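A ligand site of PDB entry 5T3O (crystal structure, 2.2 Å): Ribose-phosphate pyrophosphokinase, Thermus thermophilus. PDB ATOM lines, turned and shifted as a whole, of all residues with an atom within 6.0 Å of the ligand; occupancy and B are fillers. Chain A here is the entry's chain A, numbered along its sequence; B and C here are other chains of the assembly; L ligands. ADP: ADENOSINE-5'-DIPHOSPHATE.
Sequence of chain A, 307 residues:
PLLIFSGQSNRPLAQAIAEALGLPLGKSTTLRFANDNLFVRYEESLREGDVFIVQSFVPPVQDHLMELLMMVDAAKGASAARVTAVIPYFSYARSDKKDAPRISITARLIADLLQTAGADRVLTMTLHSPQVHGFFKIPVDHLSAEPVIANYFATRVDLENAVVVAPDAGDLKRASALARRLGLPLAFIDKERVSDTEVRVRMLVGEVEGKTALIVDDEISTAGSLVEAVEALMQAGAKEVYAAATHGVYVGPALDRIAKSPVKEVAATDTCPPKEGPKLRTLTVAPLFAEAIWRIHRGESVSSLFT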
ATOM      1  N   SER A  91     -33.107  14.550   4.376  1.00  0.00           N
ATOM      2  CA  SER A  91     -32.161  14.361   5.478  1.00  0.00           C
ATOM      3  C   SER A  91     -32.328  13.032   6.207  1.00  0.00           C
ATOM      4  O   SER A  91     -31.345  12.356   6.528  1.00  0.00           O
ATOM      5  CB  SER A  91     -32.286  15.531   6.458  1.00  0.00           C
ATOM      6  OG  SER A  91     -33.527  15.530   7.140  1.00  0.00           O
ATOM      7  N   TYR A  92     -33.588  12.640   6.437  1.00  0.00           N
ATOM      8  CA  TYR A  92     -33.885  11.360   7.095  1.00  0.00           C
ATOM      9  C   TYR A  92     -33.515  10.123   6.285  1.00  0.00           C
ATOM     10  O   TYR A  92     -33.550   9.023   6.810  1.00  0.00           O
ATOM     11  CB  TYR A  92     -35.352  11.278   7.509  1.00  0.00           C
ATOM     12  CG  TYR A  92     -35.669  12.117   8.722  1.00  0.00           C
ATOM     13  CD1 TYR A  92     -35.407  11.647   9.999  1.00  0.00           C
ATOM     14  CD2 TYR A  92     -36.235  13.380   8.591  1.00  0.00           C
ATOM     15  CE1 TYR A  92     -35.697  12.407  11.116  1.00  0.00           C
ATOM     16  CE2 TYR A  92     -36.539  14.140   9.708  1.00  0.00           C
ATOM     17  CZ  TYR A  92     -36.256  13.643  10.960  1.00  0.00           C
ATOM     18  OH  TYR A  92     -36.552  14.384  12.067  1.00  0.00           O
ATOM     19  N   ALA A  93     -33.127  10.301   5.018  1.00  0.00           N
ATOM     20  CA  ALA A  93     -32.396   9.250   4.299  1.00  0.00           C
ATOM     21  C   ALA A  93     -31.272   8.595   5.117  1.00  0.00           C
ATOM     22  O   ALA A  93     -31.006   7.408   4.950  1.00  0.00           O
ATOM     23  CB  ALA A  93     -31.840   9.804   2.990  1.00  0.00           C
ATOM     24  N   ARG A  94     -30.642   9.364   5.992  1.00  0.00           N
ATOM     25  CA  ARG A  94     -29.630   8.819   6.937  1.00  0.00           C
ATOM     26  C   ARG A  94     -30.192   7.854   8.007  1.00  0.00           C
ATOM     27  O   ARG A  94     -29.419   7.077   8.575  1.00  0.00           O
ATOM     28  CB  ARG A  94     -28.891   9.954   7.633  1.00  0.00           C
ATOM     29  CG  ARG A  94     -28.077  10.834   6.690  1.00  0.00           C
ATOM     30  CD  ARG A  94     -27.459  12.019   7.427  1.00  0.00           C
ATOM     31  NE  ARG A  94     -26.497  11.577   8.436  1.00  0.00           N
ATOM     32  CZ  ARG A  94     -25.764  12.394   9.198  1.00  0.00           C
ATOM     33  NH1 ARG A  94     -25.864  13.713   9.088  1.00  0.00           N
ATOM     34  NH2 ARG A  94     -24.931  11.867  10.090  1.00  0.00           N
ATOM     35  N   SER A  95     -31.487   7.921   8.299  1.00  0.00           N
ATOM     36  CA  SER A  95     -32.138   6.966   9.222  1.00  0.00           C
ATOM     37  C   SER A  95     -32.723   5.806   8.418  1.00  0.00           C
ATOM     38  O   SER A  95     -33.954   5.662   8.311  1.00  0.00           O
ATOM     39  CB  SER A  95     -33.219   7.669  10.048  1.00  0.00           C
ATOM     40  OG  SER A  95     -32.716   8.832  10.700  1.00  0.00           O
ATOM     41  N   ASP A  96     -31.836   4.968   7.877  1.00  0.00           N
ATOM     42  CA  ASP A  96     -32.215   3.897   6.931  1.00  0.00           C
ATOM     43  C   ASP A  96     -31.941   2.476   7.420  1.00  0.00           C
ATOM     44  O   ASP A  96     -32.266   1.522   6.731  1.00  0.00           O
ATOM     45  CB  ASP A  96     -31.541   4.130   5.570  1.00  0.00           C
ATOM     46  CG  ASP A  96     -30.004   4.168   5.656  1.00  0.00           C
ATOM     47  OD1 ASP A  96     -29.451   4.476   6.741  1.00  0.00           O
ATOM     48  OD2 ASP A  96     -29.354   3.908   4.620  1.00  0.00           O
ATOM     49  N   LYS A  97     -31.355   2.345   8.608  1.00  0.00           N
ATOM     50  CA  LYS A  97     -30.983   1.041   9.151  1.00  0.00           C
ATOM     51  C   LYS A  97     -31.511   0.977  10.570  1.00  0.00           C
ATOM     52  O   LYS A  97     -31.698   2.012  11.216  1.00  0.00           O
ATOM     53  CB  LYS A  97     -29.457   0.853   9.215  1.00  0.00           C
ATOM     54  CG  LYS A  97     -28.649   1.432   8.066  1.00  0.00           C
ATOM     55  CD  LYS A  97     -27.164   1.569   8.428  1.00  0.00           C
ATOM     56  CE  LYS A  97     -26.485   2.692   7.644  1.00  0.00           C
ATOM     57  NZ  LYS A  97     -26.867   4.069   8.111  1.00  0.00           N
ATOM     58  N   ASP A  99     -29.719   0.082  13.223  1.00  0.00           N
ATOM     59  CA  ASP A  99     -28.383  -0.154  13.807  1.00  0.00           C
ATOM     60  C   ASP A  99     -28.398  -0.198  15.351  1.00  0.00           C
ATOM     61  O   ASP A  99     -27.466  -0.732  15.957  1.00  0.00           O
ATOM     62  CB  ASP A  99     -27.320   0.828  13.263  1.00  0.00           C
ATOM     63  CG  ASP A  99     -27.728   2.302  13.377  1.00  0.00           C
ATOM     64  OD1 ASP A  99     -28.721   2.626  14.044  1.00  0.00           O
ATOM     65  OD2 ASP A  99     -27.038   3.148  12.768  1.00  0.00           O
ATOM     66  N   HIS A 128     -28.874   9.456   0.640  1.00  0.00           N
ATOM     67  CA  HIS A 128     -27.746   8.920   1.428  1.00  0.00           C
ATOM     68  C   HIS A 128     -27.338   7.496   1.071  1.00  0.00           C
ATOM     69  O   HIS A 128     -26.143   7.169   1.077  1.00  0.00           O
ATOM     70  CB  HIS A 128     -28.070   9.018   2.920  1.00  0.00           C
ATOM     71  CG  HIS A 128     -27.037   8.396   3.814  1.00  0.00           C
ATOM     72  ND1 HIS A 128     -25.825   8.990   4.066  1.00  0.00           N
ATOM     73  CD2 HIS A 128     -27.038   7.221   4.490  1.00  0.00           C
ATOM     74  CE1 HIS A 128     -25.116   8.206   4.869  1.00  0.00           C
ATOM     75  NE2 HIS A 128     -25.838   7.132   5.141  1.00  0.00           N
ATOM     76  N   ASP A 168     -16.194   8.234   2.761  1.00  0.00           N
ATOM     77  CA  ASP A 168     -16.951   7.082   3.253  1.00  0.00           C
ATOM     78  C   ASP A 168     -16.984   5.941   2.215  1.00  0.00           C
ATOM     79  O   ASP A 168     -17.190   6.186   1.025  1.00  0.00           O
ATOM     80  CB  ASP A 168     -18.373   7.545   3.591  1.00  0.00           C
ATOM     81  CG  ASP A 168     -19.279   6.434   4.109  1.00  0.00           C
ATOM     82  OD1 ASP A 168     -18.790   5.552   4.836  1.00  0.00           O
ATOM     83  OD2 ASP A 168     -20.491   6.461   3.786  1.00  0.00           O
ATOM     84  N   ALA A 169     -16.778   4.710   2.688  1.00  0.00           N
ATOM     85  CA  ALA A 169     -17.079   3.517   1.891  1.00  0.00           C
ATOM     86  C   ALA A 169     -18.604   3.356   1.910  1.00  0.00           C
ATOM     87  O   ALA A 169     -19.195   3.141   2.965  1.00  0.00           O
ATOM     88  CB  ALA A 169     -16.403   2.280   2.479  1.00  0.00           C
ATOM     89  N   LYS A 191     -14.776   4.926   8.752  1.00  0.00           N
ATOM     90  CA  LYS A 191     -14.847   4.687  10.212  1.00  0.00           C
ATOM     91  C   LYS A 191     -16.053   5.393  10.887  1.00  0.00           C
ATOM     92  O   LYS A 191     -16.812   6.104  10.230  1.00  0.00           O
ATOM     93  CB  LYS A 191     -13.521   5.114  10.892  1.00  0.00           C
ATOM     94  CG  LYS A 191     -12.590   3.977  11.297  1.00  0.00           C
ATOM     95  CD  LYS A 191     -11.258   3.975  10.544  1.00  0.00           C
ATOM     96  CE  LYS A 191     -10.232   3.087  11.226  1.00  0.00           C
ATOM     97  NZ  LYS A 191      -9.558   3.759  12.376  1.00  0.00           N
ATOM     98  N   GLU A 192     -16.191   5.175  12.192  1.00  0.00           N
ATOM     99  CA  GLU A 192     -17.242   5.783  13.049  1.00  0.00           C
ATOM    100  C   GLU A 192     -16.566   6.496  14.241  1.00  0.00           C
ATOM    101  O   GLU A 192     -15.394   6.201  14.499  1.00  0.00           O
ATOM    102  CB  GLU A 192     -18.285   4.721  13.484  1.00  0.00           C
ATOM    103  CG  GLU A 192     -17.766   3.343  13.907  1.00  0.00           C
ATOM    104  CD  GLU A 192     -17.114   3.318  15.280  1.00  0.00           C
ATOM    105  OE1 GLU A 192     -17.721   3.830  16.240  1.00  0.00           O
ATOM    106  OE2 GLU A 192     -16.010   2.756  15.407  1.00  0.00           O
ATOM    107  N   ARG A 193     -17.215   7.396  14.994  1.00  0.00           N
ATOM    108  CA  ARG A 193     -18.658   7.704  14.976  1.00  0.00           C
ATOM    109  C   ARG A 193     -18.862   9.231  15.097  1.00  0.00           C
ATOM    110  O   ARG A 193     -18.388   9.834  16.064  1.00  0.00           O
ATOM    111  CB  ARG A 193     -19.299   6.992  16.187  1.00  0.00           C
ATOM    112  CG  ARG A 193     -20.817   7.065  16.323  1.00  0.00           C
ATOM    113  CD  ARG A 193     -21.584   6.407  15.194  1.00  0.00           C
ATOM    114  NE  ARG A 193     -22.158   7.391  14.275  1.00  0.00           N
ATOM    115  CZ  ARG A 193     -21.828   7.577  12.991  1.00  0.00           C
ATOM    116  NH1 ARG A 193     -20.931   6.825  12.371  1.00  0.00           N
ATOM    117  NH2 ARG A 193     -22.445   8.536  12.296  1.00  0.00           N
ATOM    118  N   VAL A 194     -19.543   9.836  14.115  1.00  0.00           N
ATOM    119  CA  VAL A 194     -19.876  11.287  14.102  1.00  0.00           C
ATOM    120  C   VAL A 194     -20.609  11.762  15.373  1.00  0.00           C
ATOM    121  O   VAL A 194     -20.400  12.884  15.836  1.00  0.00           O
ATOM    122  CB  VAL A 194     -20.682  11.685  12.820  1.00  0.00           C
ATOM    123  CG1 VAL A 194     -21.342  13.052  12.923  1.00  0.00           C
ATOM    124  CG2 VAL A 194     -19.772  11.647  11.595  1.00  0.00           C
ATOM    125  N   SER A 195     -21.462  10.903  15.925  1.00  0.00           N
ATOM    126  CA  SER A 195     -22.170  11.168  17.190  1.00  0.00           C
ATOM    127  C   SER A 195     -21.412  10.640  18.431  1.00  0.00           C
ATOM    128  O   SER A 195     -22.036  10.105  19.350  1.00  0.00           O
ATOM    129  CB  SER A 195     -23.575  10.550  17.111  1.00  0.00           C
ATOM    130  OG  SER A 195     -24.383  10.977  18.192  1.00  0.00           O
ATOM    131  N   PHE B  33     -30.297  15.564  16.513  1.00  0.00           N
ATOM    132  CA  PHE B  33     -28.979  15.687  15.856  1.00  0.00           C
ATOM    133  C   PHE B  33     -28.728  17.140  15.466  1.00  0.00           C
ATOM    134  O   PHE B  33     -29.634  17.975  15.524  1.00  0.00           O
ATOM    135  CB  PHE B  33     -28.902  14.798  14.615  1.00  0.00           C
ATOM    136  CG  PHE B  33     -28.979  13.326  14.901  1.00  0.00           C
ATOM    137  CD1 PHE B  33     -27.999  12.692  15.645  1.00  0.00           C
ATOM    138  CD2 PHE B  33     -30.032  12.569  14.393  1.00  0.00           C
ATOM    139  CE1 PHE B  33     -28.058  11.327  15.893  1.00  0.00           C
ATOM    140  CE2 PHE B  33     -30.105  11.208  14.633  1.00  0.00           C
ATOM    141  CZ  PHE B  33     -29.118  10.589  15.395  1.00  0.00           C
ATOM    142  N   ASN B  35     -28.208  18.484  12.561  1.00  0.00           N
ATOM    143  CA  ASN B  35     -29.093  18.834  11.437  1.00  0.00           C
ATOM    144  C   ASN B  35     -30.594  18.983  11.801  1.00  0.00           C
ATOM    145  O   ASN B  35     -31.426  19.111  10.899  1.00  0.00           O
ATOM    146  CB  ASN B  35     -28.906  17.836  10.273  1.00  0.00           C
ATOM    147  CG  ASN B  35     -29.300  16.415  10.628  1.00  0.00           C
ATOM    148  OD1 ASN B  35     -29.718  16.138  11.746  1.00  0.00           O
ATOM    149  ND2 ASN B  35     -29.166  15.497   9.684  1.00  0.00           N
ATOM    150  N   ASN B  37     -32.582  16.753  13.074  1.00  0.00           N
ATOM    151  CA  ASN B  37     -33.328  15.520  12.843  1.00  0.00           C
ATOM    152  C   ASN B  37     -33.520  14.782  14.159  1.00  0.00           C
ATOM    153  O   ASN B  37     -32.612  14.760  15.021  1.00  0.00           O
ATOM    154  CB  ASN B  37     -32.615  14.618  11.841  1.00  0.00           C
ATOM    155  CG  ASN B  37     -32.776  15.100  10.399  1.00  0.00           C
ATOM    156  OD1 ASN B  37     -32.736  16.302  10.114  1.00  0.00           O
ATOM    157  ND2 ASN B  37     -32.986  14.163   9.502  1.00  0.00           N
ATOM    158  N   LEU B  38     -34.685  14.157  14.302  1.00  0.00           N
ATOM    159  CA  LEU B  38     -35.036  13.474  15.539  1.00  0.00           C
ATOM    160  C   LEU B  38     -34.577  12.040  15.489  1.00  0.00           C
ATOM    161  O   LEU B  38     -34.395  11.449  14.427  1.00  0.00           O
ATOM    162  CB  LEU B  38     -36.544  13.524  15.798  1.00  0.00           C
ATOM    163  CG  LEU B  38     -37.100  14.742  16.549  1.00  0.00           C
ATOM    164  CD1 LEU B  38     -36.451  16.034  16.108  1.00  0.00           C
ATOM    165  CD2 LEU B  38     -38.613  14.814  16.371  1.00  0.00           C
ATOM    166  N   PHE B  39     -34.408  11.491  16.685  1.00  0.00           N
ATOM    167  CA  PHE B  39     -34.015  10.122  16.882  1.00  0.00           C
ATOM    168  C   PHE B  39     -34.658   9.681  18.183  1.00  0.00           C
ATOM    169  O   PHE B  39     -34.705  10.456  19.131  1.00  0.00           O
ATOM    170  CB  PHE B  39     -32.497  10.025  16.969  1.00  0.00           C
ATOM    171  CG  PHE B  39     -31.977   8.626  17.135  1.00  0.00           C
ATOM    172  CD1 PHE B  39     -31.757   7.822  16.010  1.00  0.00           C
ATOM    173  CD2 PHE B  39     -31.707   8.107  18.398  1.00  0.00           C
ATOM    174  CE1 PHE B  39     -31.282   6.524  16.161  1.00  0.00           C
ATOM    175  CE2 PHE B  39     -31.232   6.809  18.549  1.00  0.00           C
ATOM    176  CZ  PHE B  39     -31.012   6.018  17.431  1.00  0.00           C
ATOM    177  N   LYS C 173     -18.515  -3.739   7.568  1.00  0.00           N
ATOM    178  CA  LYS C 173     -19.282  -3.682   8.821  1.00  0.00           C
ATOM    179  C   LYS C 173     -19.179  -5.003   9.600  1.00  0.00           C
ATOM    180  O   LYS C 173     -18.978  -5.006  10.810  1.00  0.00           O
ATOM    181  CB  LYS C 173     -20.761  -3.347   8.527  1.00  0.00           C
ATOM    182  CG  LYS C 173     -21.680  -3.201   9.740  1.00  0.00           C
ATOM    183  CD  LYS C 173     -21.917  -1.758  10.156  1.00  0.00           C
ATOM    184  CE  LYS C 173     -22.929  -1.673  11.286  1.00  0.00           C
ATOM    185  NZ  LYS C 173     -23.431  -0.293  11.523  1.00  0.00           N
HETATM  186  PB  ADP L   1     -23.180   6.092   7.243  1.00  0.00           P
HETATM  187  O1B ADP L   1     -24.026   5.510   6.134  1.00  0.00           O
HETATM  188  O2B ADP L   1     -23.551   7.500   7.647  1.00  0.00           O
HETATM  189  O3B ADP L   1     -21.702   5.866   7.066  1.00  0.00           O
HETATM  190  PA  ADP L   1     -23.224   5.515  10.010  1.00  0.00           P
HETATM  191  O1A ADP L   1     -21.856   6.153  10.033  1.00  0.00           O
HETATM  192  O2A ADP L   1     -23.453   4.257  10.833  1.00  0.00           O
HETATM  193  O3A ADP L   1     -23.589   5.157   8.491  1.00  0.00           O
HETATM  194  O5' ADP L   1     -24.290   6.666  10.399  1.00  0.00           O
HETATM  195  C5' ADP L   1     -25.534   6.403  11.051  1.00  0.00           C
HETATM  196  C4' ADP L   1     -25.508   6.955  12.478  1.00  0.00           C
HETATM  197  O4' ADP L   1     -25.784   8.361  12.429  1.00  0.00           O
HETATM  198  C3' ADP L   1     -26.546   6.325  13.408  1.00  0.00           C
HETATM  199  O3' ADP L   1     -26.002   5.324  14.265  1.00  0.00           O
HETATM  200  C2' ADP L   1     -27.086   7.500  14.216  1.00  0.00           C
HETATM  201  O2' ADP L   1     -26.398   7.661  15.468  1.00  0.00           O
HETATM  202  C1' ADP L   1     -26.857   8.692  13.304  1.00  0.00           C
HETATM  203  N9  ADP L   1     -28.067   9.043  12.505  1.00  0.00           N
HETATM  204  C8  ADP L   1     -29.072   8.225  12.122  1.00  0.00           C
HETATM  205  N7  ADP L   1     -30.010   8.901  11.420  1.00  0.00           N
HETATM  206  C5  ADP L   1     -29.605  10.184  11.341  1.00  0.00           C
HETATM  207  C6  ADP L   1     -30.119  11.423  10.737  1.00  0.00           C
HETATM  208  N6  ADP L   1     -31.276  11.410  10.068  1.00  0.00           N
HETATM  209  N1  ADP L   1     -29.396  12.575  10.861  1.00  0.00           N
HETATM  210  C2  ADP L   1     -28.218  12.582  11.527  1.00  0.00           C
HETATM  211  N3  ADP L   1     -27.693  11.480  12.110  1.00  0.00           N
HETATM  212  C4  ADP L   1     -28.322  10.275  12.045  1.00  0.00           C
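The backbone carbonyl oxygen (O) of Asn 35 of chain B sits close to the side-chain amide oxygen (OD1) of Asn 37 of chain B, at 3.2 Å. The side-chain amide nitrogen (ND2) of Asn 37 of chain B sits at hydrogen-bond distance from the side-chain hydroxyl (OG) of Ser 91. The side-chain amide nitrogen (ND2) of Asn 37 of chain B sits close to the backbone NH (N) of Tyr 92 (3.5 Å). The side-chain carboxylate (OD1) of Asp 96 lies within salt-bridge range of the side-chain amino group (NZ) of Lys 97. The backbone NH (N) of Leu 38 of chain B sits at hydrogen-bond distance from the side-chain hydroxyl (OH) of Tyr 92 (2.9 Å).
Ser 91 touches the ligand (O to N6, 3.7 Å). CA of Tyr 92 touches N6 of the ligand, 3.96 Å away. OD2 of Asp 168 touches O3B of the ligand (3.5 Å). CE2 of Phe 33 of chain B touches C4 of the ligand, at 3.3 Å. Hydrophobic or aromatic side chains that line the ligand: His 128 and Phe 33 of chain B. 12 residues have an atom within 4 Å of the ligand: Ser 91, Tyr 92, Arg 94, Ser 95, Lys 97, Asp 99, His 128, Asp 168, Arg 193, Phe 33 of chain B, Asn 35 of chain B and Asn 37 of chain B.
The guanidinium group (NH1) of Arg 193 lies within salt-bridge range of an oxygen (O1A) of the ligand, 2.6 Å away. NE2 of His 128 sits at hydrogen-bond distance from O1B of the ligand (2.6 Å). The side-chain hydroxyl (OG) of Ser 95 is in hydrogen-bond range of a nitrogen (N7) of the ligand (2.8 Å). An oxygen (O3') of the ligand lies within hydrogen-bond range of the side-chain carboxylate (OD2) of Asp 99, at 2.8 Å. A nitrogen (N1) of the ligand lies within hydrogen-bond range of the side-chain amide nitrogen (ND2) of Asn 35 of chain B, at 3.2 Å. A nitrogen (N6) of the ligand sits close to the side-chain amide nitrogen of Asn 37 of chain B, 3.3 Å away. The guanidinium group (NH2) of Arg 94 sits at hydrogen-bond distance from a nitrogen (N3) of the ligand. The side-chain amino group of Lys 97 lies within salt-bridge range of an oxygen (O1B) of the ligand, 3.7 Å away.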
